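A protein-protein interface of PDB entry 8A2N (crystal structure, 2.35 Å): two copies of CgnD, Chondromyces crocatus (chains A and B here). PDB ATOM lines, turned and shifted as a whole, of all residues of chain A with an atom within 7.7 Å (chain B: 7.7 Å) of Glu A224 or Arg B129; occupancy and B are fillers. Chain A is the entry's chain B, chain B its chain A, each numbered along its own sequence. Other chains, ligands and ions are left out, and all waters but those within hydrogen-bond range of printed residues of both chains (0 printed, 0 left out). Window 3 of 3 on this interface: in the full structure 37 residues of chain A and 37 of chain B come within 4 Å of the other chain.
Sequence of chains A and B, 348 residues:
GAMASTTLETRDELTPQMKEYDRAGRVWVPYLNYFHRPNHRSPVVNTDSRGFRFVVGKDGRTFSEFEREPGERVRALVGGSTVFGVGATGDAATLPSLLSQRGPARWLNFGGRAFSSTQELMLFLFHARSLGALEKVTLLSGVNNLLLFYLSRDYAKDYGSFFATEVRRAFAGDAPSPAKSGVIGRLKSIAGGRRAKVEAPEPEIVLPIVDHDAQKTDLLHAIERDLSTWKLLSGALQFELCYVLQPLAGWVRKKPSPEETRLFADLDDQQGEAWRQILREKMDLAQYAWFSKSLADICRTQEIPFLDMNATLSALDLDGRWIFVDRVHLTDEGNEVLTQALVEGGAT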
ATOM      1  N   SER A 117      -0.073 -13.378 -16.017  1.00  0.00           N
ATOM      2  CA  SER A 117      -1.230 -13.717 -16.834  1.00  0.00           C
ATOM      3  C   SER A 117      -1.229 -12.901 -18.117  1.00  0.00           C
ATOM      4  O   SER A 117      -1.513 -13.429 -19.196  1.00  0.00           O
ATOM      5  CB  SER A 117      -2.514 -13.503 -16.051  1.00  0.00           C
ATOM      6  OG  SER A 117      -2.688 -12.123 -15.724  1.00  0.00           O
ATOM      7  N   THR A 217      -6.272  -7.001  -3.690  1.00  0.00           N
ATOM      8  CA  THR A 217      -7.379  -7.279  -4.585  1.00  0.00           C
ATOM      9  C   THR A 217      -7.186  -6.581  -5.948  1.00  0.00           C
ATOM     10  O   THR A 217      -7.769  -7.013  -6.966  1.00  0.00           O
ATOM     11  CB  THR A 217      -8.757  -6.851  -4.010  1.00  0.00           C
ATOM     12  OG1 THR A 217      -8.877  -5.439  -4.079  1.00  0.00           O
ATOM     13  CG2 THR A 217      -8.921  -7.329  -2.582  1.00  0.00           C
ATOM     14  N   LEU A 219      -4.740  -6.950  -7.758  1.00  0.00           N
ATOM     15  CA  LEU A 219      -4.085  -7.832  -8.719  1.00  0.00           C
ATOM     16  C   LEU A 219      -5.123  -8.725  -9.373  1.00  0.00           C
ATOM     17  O   LEU A 219      -4.868  -9.265 -10.453  1.00  0.00           O
ATOM     18  CB  LEU A 219      -3.001  -8.669  -8.042  1.00  0.00           C
ATOM     19  CG  LEU A 219      -3.334  -9.759  -7.035  1.00  0.00           C
ATOM     20  CD1 LEU A 219      -3.508 -11.082  -7.791  1.00  0.00           C
ATOM     21  CD2 LEU A 219      -2.337  -9.888  -5.930  1.00  0.00           C
ATOM     22  N   LEU A 220      -6.305  -8.875  -8.760  1.00  0.00           N
ATOM     23  CA  LEU A 220      -7.357  -9.686  -9.377  1.00  0.00           C
ATOM     24  C   LEU A 220      -7.844  -9.069 -10.673  1.00  0.00           C
ATOM     25  O   LEU A 220      -8.211  -9.798 -11.606  1.00  0.00           O
ATOM     26  CB  LEU A 220      -8.547  -9.863  -8.438  1.00  0.00           C
ATOM     27  CG  LEU A 220      -8.295 -10.616  -7.133  1.00  0.00           C
ATOM     28  CD1 LEU A 220      -9.609 -10.745  -6.361  1.00  0.00           C
ATOM     29  CD2 LEU A 220      -7.643 -11.970  -7.355  1.00  0.00           C
ATOM     30  N   HIS A 221      -7.837  -7.736 -10.769  1.00  0.00           N
ATOM     31  CA  HIS A 221      -8.376  -7.071 -11.960  1.00  0.00           C
ATOM     32  C   HIS A 221      -7.678  -7.566 -13.218  1.00  0.00           C
ATOM     33  O   HIS A 221      -8.318  -7.874 -14.215  1.00  0.00           O
ATOM     34  CB  HIS A 221      -8.221  -5.550 -11.810  1.00  0.00           C
ATOM     35  CG  HIS A 221      -8.739  -4.767 -12.970  1.00  0.00           C
ATOM     36  ND1 HIS A 221     -10.043  -4.330 -13.049  1.00  0.00           N
ATOM     37  CD2 HIS A 221      -8.133  -4.355 -14.111  1.00  0.00           C
ATOM     38  CE1 HIS A 221     -10.220  -3.681 -14.188  1.00  0.00           C
ATOM     39  NE2 HIS A 221      -9.078  -3.683 -14.852  1.00  0.00           N
ATOM     40  N   ALA A 222      -6.352  -7.660 -13.184  1.00  0.00           N
ATOM     41  CA  ALA A 222      -5.626  -8.067 -14.371  1.00  0.00           C
ATOM     42  C   ALA A 222      -5.979  -9.499 -14.756  1.00  0.00           C
ATOM     43  O   ALA A 222      -6.051  -9.837 -15.946  1.00  0.00           O
ATOM     44  CB  ALA A 222      -4.115  -7.924 -14.138  1.00  0.00           C
ATOM     45  N   ILE A 223      -6.165 -10.364 -13.757  1.00  0.00           N
ATOM     46  CA  ILE A 223      -6.524 -11.748 -14.036  1.00  0.00           C
ATOM     47  C   ILE A 223      -7.907 -11.818 -14.664  1.00  0.00           C
ATOM     48  O   ILE A 223      -8.099 -12.436 -15.717  1.00  0.00           O
ATOM     49  CB  ILE A 223      -6.434 -12.576 -12.747  1.00  0.00           C
ATOM     50  CG1 ILE A 223      -5.001 -12.523 -12.218  1.00  0.00           C
ATOM     51  CG2 ILE A 223      -6.889 -14.047 -13.020  1.00  0.00           C
ATOM     52  CD1 ILE A 223      -4.800 -13.163 -10.888  1.00  0.00           C
ATOM     53  N   GLU A 224      -8.880 -11.168 -14.041  1.00  0.00           N
ATOM     54  CA  GLU A 224     -10.249 -11.159 -14.550  1.00  0.00           C
ATOM     55  C   GLU A 224     -10.320 -10.522 -15.935  1.00  0.00           C
ATOM     56  O   GLU A 224     -10.994 -11.050 -16.842  1.00  0.00           O
ATOM     57  CB  GLU A 224     -11.129 -10.438 -13.534  1.00  0.00           C
ATOM     58  CG  GLU A 224     -12.444  -9.900 -14.031  1.00  0.00           C
ATOM     59  CD  GLU A 224     -13.375  -9.564 -12.857  1.00  0.00           C
ATOM     60  OE1 GLU A 224     -14.606  -9.423 -13.075  1.00  0.00           O
ATOM     61  OE2 GLU A 224     -12.876  -9.455 -11.706  1.00  0.00           O
ATOM     62  N   ARG A 225      -9.600  -9.418 -16.137  1.00  0.00           N
ATOM     63  CA  ARG A 225      -9.590  -8.767 -17.446  1.00  0.00           C
ATOM     64  C   ARG A 225      -8.951  -9.658 -18.500  1.00  0.00           C
ATOM     65  O   ARG A 225      -9.485  -9.795 -19.594  1.00  0.00           O
ATOM     66  CB  ARG A 225      -8.839  -7.435 -17.377  1.00  0.00           C
ATOM     67  CG  ARG A 225      -9.047  -6.533 -18.573  1.00  0.00           C
ATOM     68  CD  ARG A 225      -8.030  -6.784 -19.683  1.00  0.00           C
ATOM     69  NE  ARG A 225      -6.706  -7.049 -19.173  1.00  0.00           N
ATOM     70  CZ  ARG A 225      -5.984  -6.181 -18.454  1.00  0.00           C
ATOM     71  NH1 ARG A 225      -6.465  -4.979 -18.176  1.00  0.00           N
ATOM     72  NH2 ARG A 225      -4.778  -6.523 -18.016  1.00  0.00           N
ATOM     73  N   ASP A 226      -7.813 -10.276 -18.195  1.00  0.00           N
ATOM     74  CA  ASP A 226      -7.197 -11.193 -19.153  1.00  0.00           C
ATOM     75  C   ASP A 226      -8.090 -12.403 -19.440  1.00  0.00           C
ATOM     76  O   ASP A 226      -8.234 -12.831 -20.601  1.00  0.00           O
ATOM     77  CB  ASP A 226      -5.840 -11.673 -18.633  1.00  0.00           C
ATOM     78  CG  ASP A 226      -4.811 -10.522 -18.530  1.00  0.00           C
ATOM     79  OD1 ASP A 226      -3.761 -10.708 -17.812  1.00  0.00           O
ATOM     80  OD2 ASP A 226      -5.050  -9.422 -19.144  1.00  0.00           O
ATOM     81  N   LEU A 227      -8.699 -12.980 -18.388  1.00  0.00           N
ATOM     82  CA  LEU A 227      -9.597 -14.112 -18.604  1.00  0.00           C
ATOM     83  C   LEU A 227     -10.757 -13.745 -19.515  1.00  0.00           C
ATOM     84  O   LEU A 227     -11.224 -14.586 -20.275  1.00  0.00           O
ATOM     85  CB  LEU A 227     -10.125 -14.626 -17.270  1.00  0.00           C
ATOM     86  CG  LEU A 227      -9.160 -15.521 -16.475  1.00  0.00           C
ATOM     87  CD1 LEU A 227      -9.787 -15.929 -15.163  1.00  0.00           C
ATOM     88  CD2 LEU A 227      -8.788 -16.728 -17.300  1.00  0.00           C
ATOM     89  N   SER A 228     -11.276 -12.511 -19.415  1.00  0.00           N
ATOM     90  CA  SER A 228     -12.359 -12.098 -20.297  1.00  0.00           C
ATOM     91  C   SER A 228     -11.891 -12.014 -21.734  1.00  0.00           C
ATOM     92  O   SER A 228     -12.687 -12.245 -22.650  1.00  0.00           O
ATOM     93  CB  SER A 228     -12.937 -10.763 -19.851  1.00  0.00           C
ATOM     94  OG  SER A 228     -12.028  -9.688 -20.118  1.00  0.00           O
ATOM     95  N   THR A 229     -10.614 -11.711 -21.956  1.00  0.00           N
ATOM     96  CA  THR A 229     -10.061 -11.701 -23.306  1.00  0.00           C
ATOM     97  C   THR A 229      -9.856 -13.122 -23.812  1.00  0.00           C
ATOM     98  O   THR A 229     -10.117 -13.416 -24.975  1.00  0.00           O
ATOM     99  CB  THR A 229      -8.727 -10.933 -23.314  1.00  0.00           C
ATOM    100  OG1 THR A 229      -8.939  -9.615 -22.798  1.00  0.00           O
ATOM    101  CG2 THR A 229      -8.166 -10.853 -24.734  1.00  0.00           C
ATOM    102  N   TRP A 230      -9.371 -14.007 -22.960  1.00  0.00           N
ATOM    103  CA  TRP A 230      -9.344 -15.433 -23.289  1.00  0.00           C
ATOM    104  C   TRP A 230     -10.749 -15.981 -23.657  1.00  0.00           C
ATOM    105  O   TRP A 230     -10.919 -16.721 -24.646  1.00  0.00           O
ATOM    106  CB  TRP A 230      -8.798 -16.236 -22.123  1.00  0.00           C
ATOM    107  CG  TRP A 230      -7.302 -16.286 -22.061  1.00  0.00           C
ATOM    108  CD1 TRP A 230      -6.487 -15.769 -21.065  1.00  0.00           C
ATOM    109  CD2 TRP A 230      -6.427 -16.900 -23.018  1.00  0.00           C
ATOM    110  NE1 TRP A 230      -5.158 -16.029 -21.368  1.00  0.00           N
ATOM    111  CE2 TRP A 230      -5.109 -16.743 -22.548  1.00  0.00           C
ATOM    112  CE3 TRP A 230      -6.635 -17.577 -24.187  1.00  0.00           C
ATOM    113  CZ2 TRP A 230      -4.015 -17.266 -23.228  1.00  0.00           C
ATOM    114  CZ3 TRP A 230      -5.557 -18.075 -24.868  1.00  0.00           C
ATOM    115  CH2 TRP A 230      -4.264 -17.896 -24.394  1.00  0.00           C
ATOM    116  N   MLY A 231     -11.737 -15.604 -22.864  1.00  0.00           N
ATOM    117  CA  MLY A 231     -13.127 -16.024 -23.081  1.00  0.00           C
ATOM    118  CB  MLY A 231     -14.078 -15.481 -22.036  1.00  0.00           C
ATOM    119  CG  MLY A 231     -14.877 -16.400 -21.209  1.00  0.00           C
ATOM    120  CD  MLY A 231     -15.719 -17.203 -22.051  1.00  0.00           C
ATOM    121  CE  MLY A 231     -15.951 -18.598 -21.703  1.00  0.00           C
ATOM    122  NZ  MLY A 231     -16.870 -19.334 -22.551  1.00  0.00           N
ATOM    123  CH1 MLY A 231     -16.784 -20.775 -22.223  1.00  0.00           C
ATOM    124  CH2 MLY A 231     -18.181 -18.866 -22.092  1.00  0.00           C
ATOM    125  C   MLY A 231     -13.643 -15.555 -24.425  1.00  0.00           C
ATOM    126  O   MLY A 231     -14.048 -16.292 -25.346  1.00  0.00           O
ATOM    127  N   LEU A 232     -13.179 -14.371 -24.787  1.00  0.00           N
ATOM    128  CA  LEU A 232     -13.515 -13.764 -26.068  1.00  0.00           C
ATOM    129  C   LEU A 232     -12.759 -14.458 -27.201  1.00  0.00           C
ATOM    130  O   LEU A 232     -13.293 -14.668 -28.267  1.00  0.00           O
ATOM    131  CB  LEU A 232     -13.175 -12.283 -25.977  1.00  0.00           C
ATOM    132  CG  LEU A 232     -13.384 -11.339 -27.114  1.00  0.00           C
ATOM    133  CD1 LEU A 232     -13.579  -9.919 -26.516  1.00  0.00           C
ATOM    134  CD2 LEU A 232     -12.167 -11.399 -28.066  1.00  0.00           C
ATOM    135  N   SER A 294     -10.996 -16.590  -4.800  1.00  0.00           N
ATOM    136  CA  SER A 294     -11.144 -15.435  -5.693  1.00  0.00           C
ATOM    137  C   SER A 294     -11.096 -15.850  -7.175  1.00  0.00           C
ATOM    138  O   SER A 294     -11.856 -15.353  -7.978  1.00  0.00           O
ATOM    139  CB  SER A 294     -10.040 -14.395  -5.417  1.00  0.00           C
ATOM    140  OG  SER A 294     -10.228 -13.799  -4.155  1.00  0.00           O
ATOM    141  N   LEU A 295     -10.196 -16.768  -7.518  1.00  0.00           N
ATOM    142  CA  LEU A 295     -10.114 -17.238  -8.901  1.00  0.00           C
ATOM    143  C   LEU A 295     -11.332 -18.074  -9.262  1.00  0.00           C
ATOM    144  O   LEU A 295     -11.864 -17.948 -10.378  1.00  0.00           O
ATOM    145  CB  LEU A 295      -8.831 -18.045  -9.139  1.00  0.00           C
ATOM    146  CG  LEU A 295      -7.548 -17.230  -9.097  1.00  0.00           C
ATOM    147  CD1 LEU A 295      -6.343 -18.118  -9.219  1.00  0.00           C
ATOM    148  CD2 LEU A 295      -7.553 -16.168 -10.182  1.00  0.00           C
ATOM    149  N   ASP A 297     -14.297 -17.652  -8.126  1.00  0.00           N
ATOM    150  CA  ASP A 297     -15.405 -16.722  -8.358  1.00  0.00           C
ATOM    151  C   ASP A 297     -15.313 -16.065  -9.729  1.00  0.00           C
ATOM    152  O   ASP A 297     -16.320 -15.898 -10.414  1.00  0.00           O
ATOM    153  CB  ASP A 297     -15.427 -15.646  -7.284  1.00  0.00           C
ATOM    154  CG  ASP A 297     -15.887 -16.154  -5.943  1.00  0.00           C
ATOM    155  OD1 ASP A 297     -16.544 -17.227  -5.899  1.00  0.00           O
ATOM    156  OD2 ASP A 297     -15.605 -15.472  -4.926  1.00  0.00           O
ATOM    157  N   ILE A 298     -14.113 -15.674 -10.139  1.00  0.00           N
ATOM    158  CA  ILE A 298     -13.932 -15.078 -11.457  1.00  0.00           C
ATOM    159  C   ILE A 298     -14.328 -16.081 -12.528  1.00  0.00           C
ATOM    160  O   ILE A 298     -15.060 -15.758 -13.464  1.00  0.00           O
ATOM    161  CB  ILE A 298     -12.471 -14.610 -11.626  1.00  0.00           C
ATOM    162  CG1 ILE A 298     -12.178 -13.472 -10.656  1.00  0.00           C
ATOM    163  CG2 ILE A 298     -12.177 -14.184 -13.054  1.00  0.00           C
ATOM    164  CD1 ILE A 298     -10.663 -13.228 -10.454  1.00  0.00           C
ATOM    165  N   CYS A 299     -13.845 -17.321 -12.400  1.00  0.00           N
ATOM    166  CA  CYS A 299     -14.094 -18.332 -13.427  1.00  0.00           C
ATOM    167  C   CYS A 299     -15.563 -18.732 -13.477  1.00  0.00           C
ATOM    168  O   CYS A 299     -16.109 -18.985 -14.556  1.00  0.00           O
ATOM    169  CB  CYS A 299     -13.226 -19.547 -13.184  1.00  0.00           C
ATOM    170  SG  CYS A 299     -11.488 -19.215 -13.544  1.00  0.00           S
ATOM    171  N   THR A 301     -18.122 -16.709 -12.730  1.00  0.00           N
ATOM    172  CA  THR A 301     -18.796 -15.583 -13.368  1.00  0.00           C
ATOM    173  C   THR A 301     -18.669 -15.637 -14.887  1.00  0.00           C
ATOM    174  O   THR A 301     -19.641 -15.419 -15.602  1.00  0.00           O
ATOM    175  CB  THR A 301     -18.212 -14.262 -12.863  1.00  0.00           C
ATOM    176  OG1 THR A 301     -18.350 -14.187 -11.445  1.00  0.00           O
ATOM    177  CG2 THR A 301     -18.945 -13.083 -13.505  1.00  0.00           C
ATOM    178  N   GLN A 302     -17.492 -15.955 -15.395  1.00  0.00           N
ATOM    179  CA  GLN A 302     -17.265 -16.038 -16.826  1.00  0.00           C
ATOM    180  C   GLN A 302     -17.548 -17.422 -17.394  1.00  0.00           C
ATOM    181  O   GLN A 302     -17.287 -17.661 -18.578  1.00  0.00           O
ATOM    182  CB  GLN A 302     -15.820 -15.616 -17.128  1.00  0.00           C
ATOM    183  CG  GLN A 302     -15.480 -14.302 -16.451  1.00  0.00           C
ATOM    184  CD  GLN A 302     -14.393 -13.523 -17.146  1.00  0.00           C
ATOM    185  OE1 GLN A 302     -14.281 -13.555 -18.368  1.00  0.00           O
ATOM    186  NE2 GLN A 302     -13.592 -12.816 -16.366  1.00  0.00           N
ATOM    187  N   ILE A 304     -16.110 -20.221 -16.947  1.00  0.00           N
ATOM    188  CA  ILE A 304     -14.869 -20.863 -17.332  1.00  0.00           C
ATOM    189  C   ILE A 304     -14.626 -22.044 -16.334  1.00  0.00           C
ATOM    190  O   ILE A 304     -14.587 -21.791 -15.146  1.00  0.00           O
ATOM    191  CB  ILE A 304     -13.682 -19.892 -17.298  1.00  0.00           C
ATOM    192  CG1 ILE A 304     -13.881 -18.782 -18.332  1.00  0.00           C
ATOM    193  CG2 ILE A 304     -12.393 -20.605 -17.562  1.00  0.00           C
ATOM    194  CD1 ILE A 304     -12.852 -17.650 -18.222  1.00  0.00           C
ATOM    195  N   PHE B  66     -14.377   6.784 -19.681  1.00  0.00           N
ATOM    196  CA  PHE B  66     -15.215   5.741 -20.259  1.00  0.00           C
ATOM    197  C   PHE B  66     -16.687   5.890 -19.867  1.00  0.00           C
ATOM    198  O   PHE B  66     -17.445   4.916 -19.893  1.00  0.00           O
ATOM    199  CB  PHE B  66     -14.700   4.342 -19.871  1.00  0.00           C
ATOM    200  CG  PHE B  66     -13.300   4.037 -20.357  1.00  0.00           C
ATOM    201  CD1 PHE B  66     -12.833   4.547 -21.538  1.00  0.00           C
ATOM    202  CD2 PHE B  66     -12.457   3.227 -19.603  1.00  0.00           C
ATOM    203  CE1 PHE B  66     -11.534   4.281 -21.987  1.00  0.00           C
ATOM    204  CE2 PHE B  66     -11.158   2.920 -20.046  1.00  0.00           C
ATOM    205  CZ  PHE B  66     -10.704   3.457 -21.233  1.00  0.00           C
ATOM    206  N   PHE B 124      -6.463  -1.166 -26.668  1.00  0.00           N
ATOM    207  CA  PHE B 124      -7.870  -1.565 -26.760  1.00  0.00           C
ATOM    208  C   PHE B 124      -8.146  -2.823 -25.948  1.00  0.00           C
ATOM    209  O   PHE B 124      -9.156  -2.914 -25.237  1.00  0.00           O
ATOM    210  CB  PHE B 124      -8.244  -1.772 -28.226  1.00  0.00           C
ATOM    211  CG  PHE B 124      -9.670  -2.132 -28.439  1.00  0.00           C
ATOM    212  CD1 PHE B 124     -10.637  -1.150 -28.505  1.00  0.00           C
ATOM    213  CD2 PHE B 124     -10.055  -3.478 -28.572  1.00  0.00           C
ATOM    214  CE1 PHE B 124     -11.974  -1.493 -28.674  1.00  0.00           C
ATOM    215  CE2 PHE B 124     -11.386  -3.821 -28.755  1.00  0.00           C
ATOM    216  CZ  PHE B 124     -12.344  -2.848 -28.796  1.00  0.00           C
ATOM    217  N   LEU B 125      -7.278  -3.819 -26.034  1.00  0.00           N
ATOM    218  CA  LEU B 125      -7.505  -5.049 -25.260  1.00  0.00           C
ATOM    219  C   LEU B 125      -7.479  -4.786 -23.760  1.00  0.00           C
ATOM    220  O   LEU B 125      -8.249  -5.397 -23.006  1.00  0.00           O
ATOM    221  CB  LEU B 125      -6.468  -6.099 -25.606  1.00  0.00           C
ATOM    222  CG  LEU B 125      -6.669  -6.792 -26.951  1.00  0.00           C
ATOM    223  CD1 LEU B 125      -5.423  -7.570 -27.332  1.00  0.00           C
ATOM    224  CD2 LEU B 125      -7.844  -7.725 -26.918  1.00  0.00           C
ATOM    225  N   PHE B 126      -6.638  -3.856 -23.303  1.00  0.00           N
ATOM    226  CA  PHE B 126      -6.557  -3.573 -21.866  1.00  0.00           C
ATOM    227  C   PHE B 126      -7.813  -2.900 -21.318  1.00  0.00           C
ATOM    228  O   PHE B 126      -8.101  -3.035 -20.122  1.00  0.00           O
ATOM    229  CB  PHE B 126      -5.361  -2.687 -21.555  1.00  0.00           C
ATOM    230  CG  PHE B 126      -4.076  -3.429 -21.444  1.00  0.00           C
ATOM    231  CD1 PHE B 126      -3.905  -4.386 -20.487  1.00  0.00           C
ATOM    232  CD2 PHE B 126      -3.013  -3.138 -22.285  1.00  0.00           C
ATOM    233  CE1 PHE B 126      -2.690  -5.070 -20.368  1.00  0.00           C
ATOM    234  CE2 PHE B 126      -1.816  -3.838 -22.185  1.00  0.00           C
ATOM    235  CZ  PHE B 126      -1.671  -4.812 -21.235  1.00  0.00           C
ATOM    236  N   HIS B 127      -8.583  -2.228 -22.166  1.00  0.00           N
ATOM    237  CA  HIS B 127      -9.705  -1.436 -21.705  1.00  0.00           C
ATOM    238  C   HIS B 127     -11.033  -1.789 -22.358  1.00  0.00           C
ATOM    239  O   HIS B 127     -12.066  -1.194 -22.014  1.00  0.00           O
ATOM    240  CB  HIS B 127      -9.400   0.058 -21.936  1.00  0.00           C
ATOM    241  CG  HIS B 127      -8.180   0.545 -21.213  1.00  0.00           C
ATOM    242  ND1 HIS B 127      -8.177   0.817 -19.865  1.00  0.00           N
ATOM    243  CD2 HIS B 127      -6.921   0.793 -21.650  1.00  0.00           C
ATOM    244  CE1 HIS B 127      -6.976   1.225 -19.503  1.00  0.00           C
ATOM    245  NE2 HIS B 127      -6.190   1.201 -20.564  1.00  0.00           N
ATOM    246  N   ALA B 128     -11.046  -2.733 -23.279  1.00  0.00           N
ATOM    247  CA  ALA B 128     -12.277  -3.036 -24.018  1.00  0.00           C
ATOM    248  C   ALA B 128     -13.445  -3.356 -23.086  1.00  0.00           C
ATOM    249  O   ALA B 128     -14.595  -3.019 -23.357  1.00  0.00           O
ATOM    250  CB  ALA B 128     -12.043  -4.226 -24.967  1.00  0.00           C
ATOM    251  N   ARG B 129     -13.167  -4.014 -21.987  1.00  0.00           N
ATOM    252  CA  ARG B 129     -14.229  -4.463 -21.101  1.00  0.00           C
ATOM    253  C   ARG B 129     -14.861  -3.324 -20.330  1.00  0.00           C
ATOM    254  O   ARG B 129     -15.944  -3.512 -19.755  1.00  0.00           O
ATOM    255  CB  ARG B 129     -13.624  -5.532 -20.178  1.00  0.00           C
ATOM    256  CG  ARG B 129     -14.553  -6.186 -19.201  1.00  0.00           C
ATOM    257  CD  ARG B 129     -13.873  -7.448 -18.714  1.00  0.00           C
ATOM    258  NE  ARG B 129     -14.582  -8.096 -17.613  1.00  0.00           N
ATOM    259  CZ  ARG B 129     -14.377  -7.798 -16.337  1.00  0.00           C
ATOM    260  NH1 ARG B 129     -13.485  -6.860 -16.015  1.00  0.00           N
ATOM    261  NH2 ARG B 129     -15.067  -8.432 -15.388  1.00  0.00           N
ATOM    262  N   SER B 130     -14.274  -2.139 -20.370  1.00  0.00           N
ATOM    263  CA  SER B 130     -14.790  -0.986 -19.638  1.00  0.00           C
ATOM    264  C   SER B 130     -15.599  -0.070 -20.582  1.00  0.00           C
ATOM    265  O   SER B 130     -16.130   0.944 -20.146  1.00  0.00           O
ATOM    266  CB  SER B 130     -13.588  -0.167 -19.138  1.00  0.00           C
ATOM    267  OG  SER B 130     -12.749  -0.980 -18.345  1.00  0.00           O
ATOM    268  N   LEU B 131     -15.658  -0.371 -21.881  1.00  0.00           N
ATOM    269  CA  LEU B 131     -16.188   0.568 -22.871  1.00  0.00           C
ATOM    270  C   LEU B 131     -17.668   0.364 -23.193  1.00  0.00           C
ATOM    271  O   LEU B 131     -18.313   1.303 -23.688  1.00  0.00           O
ATOM    272  CB  LEU B 131     -15.411   0.460 -24.189  1.00  0.00           C
ATOM    273  CG  LEU B 131     -13.886   0.396 -24.042  1.00  0.00           C
ATOM    274  CD1 LEU B 131     -13.206   0.275 -25.399  1.00  0.00           C
ATOM    275  CD2 LEU B 131     -13.409   1.630 -23.301  1.00  0.00           C
ATOM    276  N   GLY B 132     -18.216  -0.822 -22.932  1.00  0.00           N
ATOM    277  CA  GLY B 132     -19.556  -1.145 -23.377  1.00  0.00           C
ATOM    278  C   GLY B 132     -19.528  -1.676 -24.797  1.00  0.00           C
ATOM    279  O   GLY B 132     -18.486  -2.088 -25.323  1.00  0.00           O
ATOM    280  N   ALA B 133     -20.701  -1.654 -25.429  1.00  0.00           N
ATOM    281  CA  ALA B 133     -20.834  -2.141 -26.795  1.00  0.00           C
ATOM    282  C   ALA B 133     -20.431  -1.054 -27.787  1.00  0.00           C
ATOM    283  O   ALA B 133     -20.878   0.088 -27.680  1.00  0.00           O
ATOM    284  CB  ALA B 133     -22.269  -2.584 -27.061  1.00  0.00           C
ATOM    285  N   LEU B 237     -16.903  -8.985 -30.416  1.00  0.00           N
ATOM    286  CA  LEU B 237     -17.542  -7.826 -29.801  1.00  0.00           C
ATOM    287  C   LEU B 237     -18.554  -7.159 -30.727  1.00  0.00           C
ATOM    288  O   LEU B 237     -19.137  -6.138 -30.354  1.00  0.00           O
ATOM    289  CB  LEU B 237     -16.481  -6.815 -29.375  1.00  0.00           C
ATOM    290  CG  LEU B 237     -15.549  -7.289 -28.255  1.00  0.00           C
ATOM    291  CD1 LEU B 237     -14.360  -6.372 -28.045  1.00  0.00           C
ATOM    292  CD2 LEU B 237     -16.333  -7.428 -26.945  1.00  0.00           C
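O of Glu A224 sits at hydrogen-bond distance from NE2 of Gln A302, at 3.2 Å. NE of Arg A225 is in salt-bridge range of OD2 of Asp A226. The side-chain hydroxyl of Ser A228 lies within hydrogen-bond range of the backbone carbonyl oxygen of Arg A225 (2.6 Å). The side-chain hydroxyl (OG1) of Thr A229 sits at hydrogen-bond distance from the backbone carbonyl oxygen (O) of Arg A225 (3.3 Å). The backbone NH (N) of Ser A228 sits close to the side-chain amide oxygen (OE1) of Gln A302 (3.3 Å).
CD of Arg A225 touches O of Leu B125 (3.6 Å). Ser A228 touches Arg B129 (OG to CD, 3.2 Å). Leu B125 touches Thr A229. Leu B237 touches Leu A232 (CG to CD1, 3.7 Å).
No position is printed for both chains. Of the 6 pairs that touch across the chains among the printed residues, none has its exchanged pair printed and touching as well.
Of chain B, only Arg B129 (2.6 Å) comes within 4 Å of Glu A224. Printed residues of chain B within 4 Å of Arg A225: Leu B125 and Phe B126. Asp A297 touches none of the printed residues of chain B. Of the printed residues of chain A, Leu B125 touches Arg A225 (3.6 Å) and Thr A229 (3.8 Å). Of chain A, only Glu A224 and Ser A228 come within 4 Å of Arg B129. The nearest printed residue of chain B that does not touch Glu A224 is Leu B125 (8.8 Å). The nearest printed residue of chain B that does not touch Ser A228 is Leu B125 (6.4 Å).
Of the 24 printed residues of chain A, 5 touch a printed residue of chain B. Printed residues of chain A that touch a printed residue of chain B: Glu A224, Arg A225, Ser A228, Thr A229 and Leu A232. Along chain A the printed residues that touch a printed residue of chain B span positions 224 to 232. Among the printed residues, 6 pairs touch across the chains. Among the printed residues, Asp or Glu carboxylates within 4 Å of a Lys or Arg side-chain nitrogen of the other chain: Glu A224 with Arg B129.
The side-chain carboxylate (OE1) of Glu A224 is in salt-bridge range of the guanidinium group (NH2) of Arg B129 (2.6 Å). The guanidinium group (NH1) of Arg A225 lies within hydrogen-bond range of the backbone carbonyl oxygen (O) of Phe B126, at 3.2 Å.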
